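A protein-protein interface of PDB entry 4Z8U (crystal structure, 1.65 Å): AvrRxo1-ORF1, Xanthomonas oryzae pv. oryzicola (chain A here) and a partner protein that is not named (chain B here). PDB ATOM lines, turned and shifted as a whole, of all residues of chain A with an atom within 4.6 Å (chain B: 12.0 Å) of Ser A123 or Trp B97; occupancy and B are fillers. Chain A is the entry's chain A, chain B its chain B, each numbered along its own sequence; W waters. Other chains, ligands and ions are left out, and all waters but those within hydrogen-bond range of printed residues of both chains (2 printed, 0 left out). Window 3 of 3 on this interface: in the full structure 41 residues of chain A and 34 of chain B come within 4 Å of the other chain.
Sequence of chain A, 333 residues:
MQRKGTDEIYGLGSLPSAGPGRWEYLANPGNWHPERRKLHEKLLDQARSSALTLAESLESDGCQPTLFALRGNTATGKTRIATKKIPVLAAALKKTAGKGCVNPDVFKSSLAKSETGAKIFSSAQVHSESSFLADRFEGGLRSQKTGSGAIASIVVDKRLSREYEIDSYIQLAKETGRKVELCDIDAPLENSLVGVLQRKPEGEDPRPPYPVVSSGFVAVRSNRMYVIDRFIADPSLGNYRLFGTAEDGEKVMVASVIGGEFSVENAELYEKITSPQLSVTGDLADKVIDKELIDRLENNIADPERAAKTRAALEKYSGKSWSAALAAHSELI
Water W2 bridges the backbone carbonyl oxygen (O) of Ser B96 (2.6 Å) and the backbone carbonyl oxygen (O) of Ser A123 (3.2 Å). Water W1 bridges the backbone carbonyl oxygen of Ala A124 (2.8 Å) and the side-chain hydroxyl of Ser B96 (3.0 Å).
No residue of chain B comes within 4 Å of Ser A122. Ser A123 touches just one residue of chain B: Trp B97 (3.9 Å). No residue of chain B comes within 4 Å of Gln A125. His A127 touches just these residues of chain B: Phe B95 (3.3 Å), Ser B96 (3.2 Å), Trp B97 (3.6 Å) and Ser B98 (3.6 Å). Printed residues of chain B within 4 Å of Pro A208: Trp B97. Of the printed residues of chain B, Val A212 touches Thr B93 (3.98 Å), Leu B94 (3.7 Å), Trp B97 (3.7 Å) and Ser B98 (3.7 Å). Of chain B, only Trp B97 (3.1 Å) comes within 4 Å of Ser A330. Tyr B70 touches none of the printed residues of chain A. Of the printed residues of chain A, Leu B94 touches Val A212. Printed residues of chain A within 4 Å of Ser B96: Ala A124 (3.9 Å) and His A127 (3.2 Å). Of the printed residues of chain A, Trp B97 touches Ser A123, His A127, Arg A207, Pro A208, Pro A209, Val A212 and Ser A330.
ND1 of His A127 is in hydrogen-bond range of NZ of Lys A108 (3.0 Å). OG of Ser A122 sits close to N of Ala A124, at 3.5 Å. OG of Ser A330 lies within hydrogen-bond range of O of Arg A207. O of His B89 sits at hydrogen-bond distance from OG1 of Thr B93 (3.0 Å). O of Glu B92 is in hydrogen-bond range of OG of Ser B96.
Among the printed residues, merely in contact across the chains: Ser A123 with Trp B97 (3.9 Å), Ala A124 with Ser B96 (3.9 Å), His A127 with Phe B95 (3.3 Å), His A127 with Ser B96 (3.2 Å), His A127 with Trp B97 (3.6 Å), His A127 with Ser B98 (3.6 Å), Arg A207 with Trp B97 (3.3 Å), Pro A208 with Trp B97 (3.6 Å), Pro A209 with Thr B93 (3.6 Å), Pro A209 with Trp B97 (3.3 Å), Val A212 with Thr B93 (3.98 Å), Val A212 with Leu B94 (3.7 Å), Val A212 with Trp B97 (3.7 Å), Val A212 with Ser B98 (3.7 Å) and Ser A330 with Trp B97 (3.1 Å).
Of the 13 printed residues of chain A, 8 touch a printed residue of chain B. Hydrophobic or aromatic side chains of chain A that line the printed part of chain B: His A127, Pro A208, Pro A209 and Val A212. Hydrophobic or aromatic side chains of chain B that line the printed part of chain A: Leu B94 and Trp B97. Among the printed residues, 15 pairs touch across the chains.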
ATOM      1  N   LYS A 108      -9.374 -27.534  32.635  1.00  0.00           N
ATOM      2  CA  LYS A 108      -9.697 -26.434  31.695  1.00  0.00           C
ATOM      3  C   LYS A 108     -10.968 -25.762  32.001  1.00  0.00           C
ATOM      4  O   LYS A 108     -11.014 -24.521  31.938  1.00  0.00           O
ATOM      5  CB  LYS A 108      -9.682 -26.909  30.224  1.00  0.00           C
ATOM      6  CG  LYS A 108      -8.271 -27.167  29.694  1.00  0.00           C
ATOM      7  CD  LYS A 108      -8.367 -27.543  28.179  1.00  0.00           C
ATOM      8  CE  LYS A 108      -7.032 -27.401  27.479  1.00  0.00           C
ATOM      9  NZ  LYS A 108      -6.145 -28.458  28.008  1.00  0.00           N
ATOM     10  N   PHE A 121     -12.850 -17.789  29.071  1.00  0.00           N
ATOM     11  CA  PHE A 121     -11.696 -18.000  28.256  1.00  0.00           C
ATOM     12  C   PHE A 121     -11.956 -19.273  27.399  1.00  0.00           C
ATOM     13  O   PHE A 121     -12.678 -20.181  27.852  1.00  0.00           O
ATOM     14  CB  PHE A 121     -10.458 -18.289  29.119  1.00  0.00           C
ATOM     15  CG  PHE A 121     -10.070 -17.125  29.950  1.00  0.00           C
ATOM     16  CD1 PHE A 121      -9.688 -15.919  29.329  1.00  0.00           C
ATOM     17  CD2 PHE A 121     -10.062 -17.220  31.373  1.00  0.00           C
ATOM     18  CE1 PHE A 121      -9.300 -14.866  30.119  1.00  0.00           C
ATOM     19  CE2 PHE A 121      -9.731 -16.111  32.145  1.00  0.00           C
ATOM     20  CZ  PHE A 121      -9.356 -14.957  31.525  1.00  0.00           C
ATOM     21  N   SER A 122     -11.335 -19.331  26.248  1.00  0.00           N
ATOM     22  CA  SER A 122     -11.479 -20.541  25.419  1.00  0.00           C
ATOM     23  C   SER A 122     -10.521 -21.621  25.917  1.00  0.00           C
ATOM     24  O   SER A 122      -9.557 -21.327  26.659  1.00  0.00           O
ATOM     25  CB  SER A 122     -11.122 -20.199  23.996  1.00  0.00           C
ATOM     26  OG  SER A 122      -9.706 -19.949  23.858  1.00  0.00           O
ATOM     27  N   SER A 123     -10.765 -22.852  25.462  1.00  0.00           N
ATOM     28  CA  SER A 123      -9.867 -23.956  25.789  1.00  0.00           C
ATOM     29  C   SER A 123      -8.450 -23.629  25.402  1.00  0.00           C
ATOM     30  O   SER A 123      -7.540 -23.958  26.133  1.00  0.00           O
ATOM     31  CB  SER A 123     -10.271 -25.216  25.007  1.00  0.00           C
ATOM     32  OG  SER A 123     -11.256 -25.884  25.747  1.00  0.00           O
ATOM     33  N   ALA A 124      -8.226 -23.066  24.204  1.00  0.00           N
ATOM     34  CA  ALA A 124      -6.859 -22.776  23.776  1.00  0.00           C
ATOM     35  C   ALA A 124      -6.224 -21.724  24.684  1.00  0.00           C
ATOM     36  O   ALA A 124      -4.999 -21.759  24.957  1.00  0.00           O
ATOM     37  CB  ALA A 124      -6.812 -22.310  22.305  1.00  0.00           C
ATOM     38  N   GLN A 125      -7.069 -20.772  25.147  1.00  0.00           N
ATOM     39  CA  GLN A 125      -6.559 -19.716  26.011  1.00  0.00           C
ATOM     40  C   GLN A 125      -6.067 -20.284  27.362  1.00  0.00           C
ATOM     41  O   GLN A 125      -5.105 -19.713  27.940  1.00  0.00           O
ATOM     42  CB  GLN A 125      -7.687 -18.699  26.309  1.00  0.00           C
ATOM     43  CG  GLN A 125      -7.789 -17.631  25.174  1.00  0.00           C
ATOM     44  CD  GLN A 125      -8.772 -16.595  25.609  1.00  0.00           C
ATOM     45  OE1 GLN A 125      -9.913 -16.893  25.696  1.00  0.00           O
ATOM     46  NE2 GLN A 125      -8.285 -15.383  25.984  1.00  0.00           N
ATOM     47  N   VAL A 126      -6.682 -21.372  27.824  1.00  0.00           N
ATOM     48  CA  VAL A 126      -6.294 -21.946  29.108  1.00  0.00           C
ATOM     49  C   VAL A 126      -5.293 -23.147  28.979  1.00  0.00           C
ATOM     50  O   VAL A 126      -4.926 -23.746  29.992  1.00  0.00           O
ATOM     51  CB  VAL A 126      -7.480 -22.337  30.027  1.00  0.00           C
ATOM     52  CG1 VAL A 126      -8.269 -21.029  30.470  1.00  0.00           C
ATOM     53  CG2 VAL A 126      -8.391 -23.411  29.416  1.00  0.00           C
ATOM     54  N   HIS A 127      -4.933 -23.526  27.754  1.00  0.00           N
ATOM     55  CA  HIS A 127      -4.220 -24.826  27.611  1.00  0.00           C
ATOM     56  C   HIS A 127      -2.857 -24.819  28.253  1.00  0.00           C
ATOM     57  O   HIS A 127      -2.503 -25.808  28.978  1.00  0.00           O
ATOM     58  CB  HIS A 127      -4.132 -25.245  26.144  1.00  0.00           C
ATOM     59  CG  HIS A 127      -3.276 -26.485  25.969  1.00  0.00           C
ATOM     60  ND1 HIS A 127      -3.716 -27.712  26.373  1.00  0.00           N
ATOM     61  CD2 HIS A 127      -2.000 -26.645  25.540  1.00  0.00           C
ATOM     62  CE1 HIS A 127      -2.748 -28.636  26.169  1.00  0.00           C
ATOM     63  NE2 HIS A 127      -1.702 -28.003  25.657  1.00  0.00           N
ATOM     64  N   ARG A 207     -12.630 -30.180  22.300  1.00  0.00           N
ATOM     65  CA  ARG A 207     -13.112 -30.073  20.895  1.00  0.00           C
ATOM     66  C   ARG A 207     -12.004 -29.447  20.054  1.00  0.00           C
ATOM     67  O   ARG A 207     -12.065 -28.273  19.665  1.00  0.00           O
ATOM     68  CB  ARG A 207     -14.362 -29.199  20.835  1.00  0.00           C
ATOM     69  CG  ARG A 207     -15.597 -29.862  21.474  1.00  0.00           C
ATOM     70  CD  ARG A 207     -16.704 -28.810  21.764  1.00  0.00           C
ATOM     71  NE  ARG A 207     -16.307 -27.941  22.878  1.00  0.00           N
ATOM     72  CZ  ARG A 207     -16.008 -26.644  22.768  1.00  0.00           C
ATOM     73  NH1 ARG A 207     -16.020 -26.024  21.582  1.00  0.00           N
ATOM     74  NH2 ARG A 207     -15.726 -25.904  23.874  1.00  0.00           N
ATOM     75  N   PRO A 208     -10.955 -30.221  19.727  1.00  0.00           N
ATOM     76  CA  PRO A 208      -9.888 -29.613  18.975  1.00  0.00           C
ATOM     77  C   PRO A 208     -10.157 -29.472  17.527  1.00  0.00           C
ATOM     78  O   PRO A 208     -11.096 -30.128  17.009  1.00  0.00           O
ATOM     79  CB  PRO A 208      -8.744 -30.614  19.184  1.00  0.00           C
ATOM     80  CG  PRO A 208      -9.398 -31.972  19.390  1.00  0.00           C
ATOM     81  CD  PRO A 208     -10.647 -31.620  20.163  1.00  0.00           C
ATOM     82  N   PRO A 209      -9.378 -28.639  16.832  1.00  0.00           N
ATOM     83  CA  PRO A 209      -9.517 -28.532  15.362  1.00  0.00           C
ATOM     84  C   PRO A 209      -8.880 -29.719  14.630  1.00  0.00           C
ATOM     85  O   PRO A 209      -8.195 -30.576  15.283  1.00  0.00           O
ATOM     86  CB  PRO A 209      -8.781 -27.238  15.064  1.00  0.00           C
ATOM     87  CG  PRO A 209      -7.676 -27.244  16.065  1.00  0.00           C
ATOM     88  CD  PRO A 209      -8.235 -27.817  17.355  1.00  0.00           C
ATOM     89  N   VAL A 212      -5.039 -31.205  14.953  1.00  0.00           N
ATOM     90  CA  VAL A 212      -4.790 -31.962  16.187  1.00  0.00           C
ATOM     91  C   VAL A 212      -5.201 -33.422  16.050  1.00  0.00           C
ATOM     92  O   VAL A 212      -4.466 -34.376  16.402  1.00  0.00           O
ATOM     93  CB  VAL A 212      -5.574 -31.273  17.356  1.00  0.00           C
ATOM     94  CG1 VAL A 212      -5.542 -32.160  18.642  1.00  0.00           C
ATOM     95  CG2 VAL A 212      -4.932 -29.890  17.629  1.00  0.00           C
ATOM     96  N   SER A 330     -14.637 -26.068  17.228  1.00  0.00           N
ATOM     97  CA  SER A 330     -13.677 -25.871  18.232  1.00  0.00           C
ATOM     98  C   SER A 330     -13.759 -24.445  18.825  1.00  0.00           C
ATOM     99  O   SER A 330     -13.367 -24.220  20.000  1.00  0.00           O
ATOM    100  CB  SER A 330     -12.304 -26.047  17.623  1.00  0.00           C
ATOM    101  OG  SER A 330     -11.333 -25.894  18.629  1.00  0.00           O
ATOM    102  N   ASP B  53       7.219 -22.649  18.941  1.00  0.00           N
ATOM    103  CA  ASP B  53       7.896 -23.436  19.940  1.00  0.00           C
ATOM    104  C   ASP B  53       7.661 -24.920  19.635  1.00  0.00           C
ATOM    105  O   ASP B  53       6.514 -25.369  19.574  1.00  0.00           O
ATOM    106  CB  ASP B  53       7.316 -23.019  21.312  1.00  0.00           C
ATOM    107  CG  ASP B  53       7.588 -24.016  22.424  1.00  0.00           C
ATOM    108  OD1 ASP B  53       8.627 -24.717  22.404  1.00  0.00           O
ATOM    109  OD2 ASP B  53       6.737 -24.034  23.357  1.00  0.00           O
ATOM    110  N   SER B  55       9.182 -27.435  21.377  1.00  0.00           N
ATOM    111  CA  SER B  55       9.845 -28.168  22.440  1.00  0.00           C
ATOM    112  C   SER B  55       8.921 -29.128  23.187  1.00  0.00           C
ATOM    113  O   SER B  55       9.431 -30.007  23.888  1.00  0.00           O
ATOM    114  CB  SER B  55      10.533 -27.199  23.434  1.00  0.00           C
ATOM    115  OG  SER B  55       9.637 -26.147  23.802  1.00  0.00           O
ATOM    116  N   ASP B  56       7.603 -28.961  23.066  1.00  0.00           N
ATOM    117  CA  ASP B  56       6.643 -29.719  23.926  1.00  0.00           C
ATOM    118  C   ASP B  56       6.900 -29.419  25.419  1.00  0.00           C
ATOM    119  O   ASP B  56       7.058 -30.340  26.272  1.00  0.00           O
ATOM    120  CB  ASP B  56       6.708 -31.251  23.697  1.00  0.00           C
ATOM    121  CG  ASP B  56       5.475 -31.983  24.275  1.00  0.00           C
ATOM    122  OD1 ASP B  56       4.541 -31.258  24.710  1.00  0.00           O
ATOM    123  OD2 ASP B  56       5.449 -33.252  24.272  1.00  0.00           O
ATOM    124  N   ALA B  57       6.990 -28.124  25.711  1.00  0.00           N
ATOM    125  CA  ALA B  57       7.263 -27.665  27.051  1.00  0.00           C
ATOM    126  C   ALA B  57       8.669 -28.090  27.518  1.00  0.00           C
ATOM    127  O   ALA B  57       8.833 -28.461  28.682  1.00  0.00           O
ATOM    128  CB  ALA B  57       6.175 -28.204  27.999  1.00  0.00           C
ATOM    129  N   ARG B  59      10.113 -30.774  27.013  1.00  0.00           N
ATOM    130  CA  ARG B  59      10.164 -32.240  26.984  1.00  0.00           C
ATOM    131  C   ARG B  59      10.980 -32.844  25.815  1.00  0.00           C
ATOM    132  O   ARG B  59      11.384 -34.005  25.894  1.00  0.00           O
ATOM    133  CB  ARG B  59       8.768 -32.747  26.799  1.00  0.00           C
ATOM    134  CG  ARG B  59       7.960 -33.032  28.022  1.00  0.00           C
ATOM    135  CD  ARG B  59       6.704 -33.631  27.400  1.00  0.00           C
ATOM    136  NE  ARG B  59       5.844 -34.211  28.406  1.00  0.00           N
ATOM    137  CZ  ARG B  59       5.935 -35.467  28.854  1.00  0.00           C
ATOM    138  NH1 ARG B  59       6.866 -36.321  28.376  1.00  0.00           N
ATOM    139  NH2 ARG B  59       5.074 -35.869  29.795  1.00  0.00           N
ATOM    140  N   TYR B  70       9.391 -33.181  13.052  1.00  0.00           N
ATOM    141  CA  TYR B  70       8.760 -32.042  12.389  1.00  0.00           C
ATOM    142  C   TYR B  70       9.005 -32.077  10.862  1.00  0.00           C
ATOM    143  O   TYR B  70       8.210 -31.574  10.087  1.00  0.00           O
ATOM    144  CB  TYR B  70       9.112 -30.652  12.993  1.00  0.00           C
ATOM    145  CG  TYR B  70       8.498 -30.501  14.401  1.00  0.00           C
ATOM    146  CD1 TYR B  70       7.112 -30.330  14.550  1.00  0.00           C
ATOM    147  CD2 TYR B  70       9.282 -30.670  15.525  1.00  0.00           C
ATOM    148  CE1 TYR B  70       6.523 -30.283  15.813  1.00  0.00           C
ATOM    149  CE2 TYR B  70       8.748 -30.596  16.786  1.00  0.00           C
ATOM    150  CZ  TYR B  70       7.358 -30.419  16.918  1.00  0.00           C
ATOM    151  OH  TYR B  70       6.839 -30.380  18.175  1.00  0.00           O
ATOM    152  N   MET B  73       6.577 -34.549   9.515  1.00  0.00           N
ATOM    153  CA  MET B  73       5.214 -33.954   9.557  1.00  0.00           C
ATOM    154  C   MET B  73       5.092 -32.958   8.406  1.00  0.00           C
ATOM    155  O   MET B  73       4.091 -32.890   7.700  1.00  0.00           O
ATOM    156  CB  MET B  73       4.944 -33.332  10.954  1.00  0.00           C
ATOM    157  CG  MET B  73       3.568 -32.729  10.933  1.00  0.00           C
ATOM    158  SD  MET B  73       3.418 -31.809  12.702  1.00  0.00           S
ATOM    159  CE  MET B  73       3.501 -33.412  13.750  1.00  0.00           C
ATOM    160  N   TYR B  78       1.674 -32.655   5.550  1.00  0.00           N
ATOM    161  CA  TYR B  78       1.137 -31.351   5.151  1.00  0.00           C
ATOM    162  C   TYR B  78       1.646 -30.973   3.768  1.00  0.00           C
ATOM    163  O   TYR B  78       2.361 -29.958   3.610  1.00  0.00           O
ATOM    164  CB  TYR B  78       1.449 -30.246   6.197  1.00  0.00           C
ATOM    165  CG  TYR B  78       0.659 -30.490   7.501  1.00  0.00           C
ATOM    166  CD1 TYR B  78      -0.701 -30.029   7.636  1.00  0.00           C
ATOM    167  CD2 TYR B  78       1.209 -31.253   8.537  1.00  0.00           C
ATOM    168  CE1 TYR B  78      -1.451 -30.366   8.741  1.00  0.00           C
ATOM    169  CE2 TYR B  78       0.498 -31.535   9.692  1.00  0.00           C
ATOM    170  CZ  TYR B  78      -0.861 -31.086   9.771  1.00  0.00           C
ATOM    171  OH  TYR B  78      -1.634 -31.363  10.873  1.00  0.00           O
ATOM    172  N   ALA B  88       4.488 -23.273  10.766  1.00  0.00           N
ATOM    173  CA  ALA B  88       4.518 -22.713  12.095  1.00  0.00           C
ATOM    174  C   ALA B  88       3.158 -22.528  12.712  1.00  0.00           C
ATOM    175  O   ALA B  88       2.981 -22.781  13.860  1.00  0.00           O
ATOM    176  CB  ALA B  88       5.204 -21.410  12.060  1.00  0.00           C
ATOM    177  N   HIS B  89       2.201 -22.055  11.956  1.00  0.00           N
ATOM    178  CA  HIS B  89       0.904 -21.872  12.515  1.00  0.00           C
ATOM    179  C   HIS B  89       0.266 -23.184  12.853  1.00  0.00           C
ATOM    180  O   HIS B  89      -0.532 -23.255  13.742  1.00  0.00           O
ATOM    181  CB  HIS B  89       0.018 -21.125  11.560  1.00  0.00           C
ATOM    182  CG  HIS B  89       0.481 -19.735  11.303  1.00  0.00           C
ATOM    183  ND1 HIS B  89       1.587 -19.210  11.921  1.00  0.00           N
ATOM    184  CD2 HIS B  89       0.016 -18.775  10.477  1.00  0.00           C
ATOM    185  CE1 HIS B  89       1.776 -17.977  11.504  1.00  0.00           C
ATOM    186  NE2 HIS B  89       0.833 -17.688  10.629  1.00  0.00           N
ATOM    187  N   ILE B  90       0.638 -24.212  12.111  1.00  0.00           N
ATOM    188  CA  ILE B  90       0.138 -25.537  12.355  1.00  0.00           C
ATOM    189  C   ILE B  90       0.737 -26.079  13.630  1.00  0.00           C
ATOM    190  O   ILE B  90       0.037 -26.598  14.438  1.00  0.00           O
ATOM    191  CB  ILE B  90       0.393 -26.454  11.203  1.00  0.00           C
ATOM    192  CG1 ILE B  90      -0.494 -26.081  10.056  1.00  0.00           C
ATOM    193  CG2 ILE B  90       0.087 -27.845  11.584  1.00  0.00           C
ATOM    194  CD1 ILE B  90       0.022 -26.487   8.784  1.00  0.00           C
ATOM    195  N   VAL B  91       2.029 -25.901  13.815  1.00  0.00           N
ATOM    196  CA  VAL B  91       2.682 -26.433  15.015  1.00  0.00           C
ATOM    197  C   VAL B  91       2.109 -25.736  16.251  1.00  0.00           C
ATOM    198  O   VAL B  91       1.865 -26.407  17.265  1.00  0.00           O
ATOM    199  CB  VAL B  91       4.205 -26.288  14.945  1.00  0.00           C
ATOM    200  CG1 VAL B  91       4.816 -26.687  16.289  1.00  0.00           C
ATOM    201  CG2 VAL B  91       4.757 -27.118  13.818  1.00  0.00           C
ATOM    202  N   GLU B  92       1.880 -24.407  16.149  1.00  0.00           N
ATOM    203  CA  GLU B  92       1.306 -23.629  17.264  1.00  0.00           C
ATOM    204  C   GLU B  92      -0.065 -24.211  17.629  1.00  0.00           C
ATOM    205  O   GLU B  92      -0.354 -24.394  18.799  1.00  0.00           O
ATOM    206  CB  GLU B  92       1.127 -22.154  16.876  1.00  0.00           C
ATOM    207  CG  GLU B  92       2.492 -21.483  16.686  1.00  0.00           C
ATOM    208  CD  GLU B  92       2.427 -20.201  15.842  1.00  0.00           C
ATOM    209  OE1 GLU B  92       1.331 -19.779  15.335  1.00  0.00           O
ATOM    210  OE2 GLU B  92       3.514 -19.597  15.660  1.00  0.00           O
ATOM    211  N   THR B  93      -0.863 -24.472  16.619  1.00  0.00           N
ATOM    212  CA  THR B  93      -2.204 -25.096  16.820  1.00  0.00           C
ATOM    213  C   THR B  93      -2.046 -26.416  17.535  1.00  0.00           C
ATOM    214  O   THR B  93      -2.770 -26.668  18.529  1.00  0.00           O
ATOM    215  CB  THR B  93      -2.893 -25.350  15.502  1.00  0.00           C
ATOM    216  OG1 THR B  93      -3.158 -24.103  14.831  1.00  0.00           O
ATOM    217  CG2 THR B  93      -4.279 -26.049  15.693  1.00  0.00           C
ATOM    218  N   LEU B  94      -1.095 -27.281  17.096  1.00  0.00           N
ATOM    219  CA  LEU B  94      -0.926 -28.587  17.763  1.00  0.00           C
ATOM    220  C   LEU B  94      -0.651 -28.512  19.242  1.00  0.00           C
ATOM    221  O   LEU B  94      -1.117 -29.347  20.057  1.00  0.00           O
ATOM    222  CB  LEU B  94       0.117 -29.458  17.075  1.00  0.00           C
ATOM    223  CG  LEU B  94      -0.135 -29.789  15.627  1.00  0.00           C
ATOM    224  CD1 LEU B  94       1.011 -30.675  15.113  1.00  0.00           C
ATOM    225  CD2 LEU B  94      -1.475 -30.523  15.444  1.00  0.00           C
ATOM    226  N   PHE B  95       0.155 -27.494  19.588  1.00  0.00           N
ATOM    227  CA  PHE B  95       0.480 -27.283  20.999  1.00  0.00           C
ATOM    228  C   PHE B  95      -0.462 -26.410  21.795  1.00  0.00           C
ATOM    229  O   PHE B  95      -0.132 -26.042  22.912  1.00  0.00           O
ATOM    230  CB  PHE B  95       1.940 -26.860  21.107  1.00  0.00           C
ATOM    231  CG  PHE B  95       2.858 -27.991  20.806  1.00  0.00           C
ATOM    232  CD1 PHE B  95       3.070 -28.996  21.727  1.00  0.00           C
ATOM    233  CD2 PHE B  95       3.431 -28.094  19.534  1.00  0.00           C
ATOM    234  CE1 PHE B  95       3.882 -30.098  21.405  1.00  0.00           C
ATOM    235  CE2 PHE B  95       4.255 -29.159  19.211  1.00  0.00           C
ATOM    236  CZ  PHE B  95       4.472 -30.175  20.139  1.00  0.00           C
ATOM    237  N   SER B  96      -1.630 -26.116  21.262  1.00  0.00           N
ATOM    238  CA  SER B  96      -2.705 -25.399  21.971  1.00  0.00           C
ATOM    239  C   SER B  96      -3.744 -26.360  22.492  1.00  0.00           C
ATOM    240  O   SER B  96      -4.736 -25.913  23.039  1.00  0.00           O
ATOM    241  CB  SER B  96      -3.386 -24.344  21.064  1.00  0.00           C
ATOM    242  OG  SER B  96      -2.395 -23.364  20.720  1.00  0.00           O
ATOM    243  N   TRP B  97      -3.545 -27.677  22.235  1.00  0.00           N
ATOM    244  CA  TRP B  97      -4.575 -28.706  22.537  1.00  0.00           C
ATOM    245  C   TRP B  97      -3.859 -29.949  23.014  1.00  0.00           C
ATOM    246  O   TRP B  97      -2.683 -30.128  22.698  1.00  0.00           O
ATOM    247  CB  TRP B  97      -5.274 -29.113  21.220  1.00  0.00           C
ATOM    248  CG  TRP B  97      -6.067 -27.961  20.717  1.00  0.00           C
ATOM    249  CD1 TRP B  97      -5.634 -26.944  19.884  1.00  0.00           C
ATOM    250  CD2 TRP B  97      -7.379 -27.622  21.116  1.00  0.00           C
ATOM    251  NE1 TRP B  97      -6.637 -26.034  19.687  1.00  0.00           N
ATOM    252  CE2 TRP B  97      -7.699 -26.384  20.431  1.00  0.00           C
ATOM    253  CE3 TRP B  97      -8.368 -28.254  21.939  1.00  0.00           C
ATOM    254  CZ2 TRP B  97      -8.936 -25.791  20.553  1.00  0.00           C
ATOM    255  CZ3 TRP B  97      -9.598 -27.627  22.034  1.00  0.00           C
ATOM    256  CH2 TRP B  97      -9.880 -26.472  21.356  1.00  0.00           C
ATOM    257  N   SER B  98      -4.519 -30.735  23.891  1.00  0.00           N
ATOM    258  CA  SER B  98      -3.918 -32.024  24.341  1.00  0.00           C
ATOM    259  C   SER B  98      -3.853 -33.074  23.159  1.00  0.00           C
ATOM    260  O   SER B  98      -4.434 -32.754  22.083  1.00  0.00           O
ATOM    261  CB  SER B  98      -4.681 -32.653  25.478  1.00  0.00           C
ATOM    262  OG  SER B  98      -6.026 -33.005  25.004  1.00  0.00           O
HETATM  263  O   HOH W   1      -2.720 -21.987  23.368  1.00  0.00           O
HETATM  264  O   HOH W   2      -6.986 -26.540  24.274  1.00  0.00           O
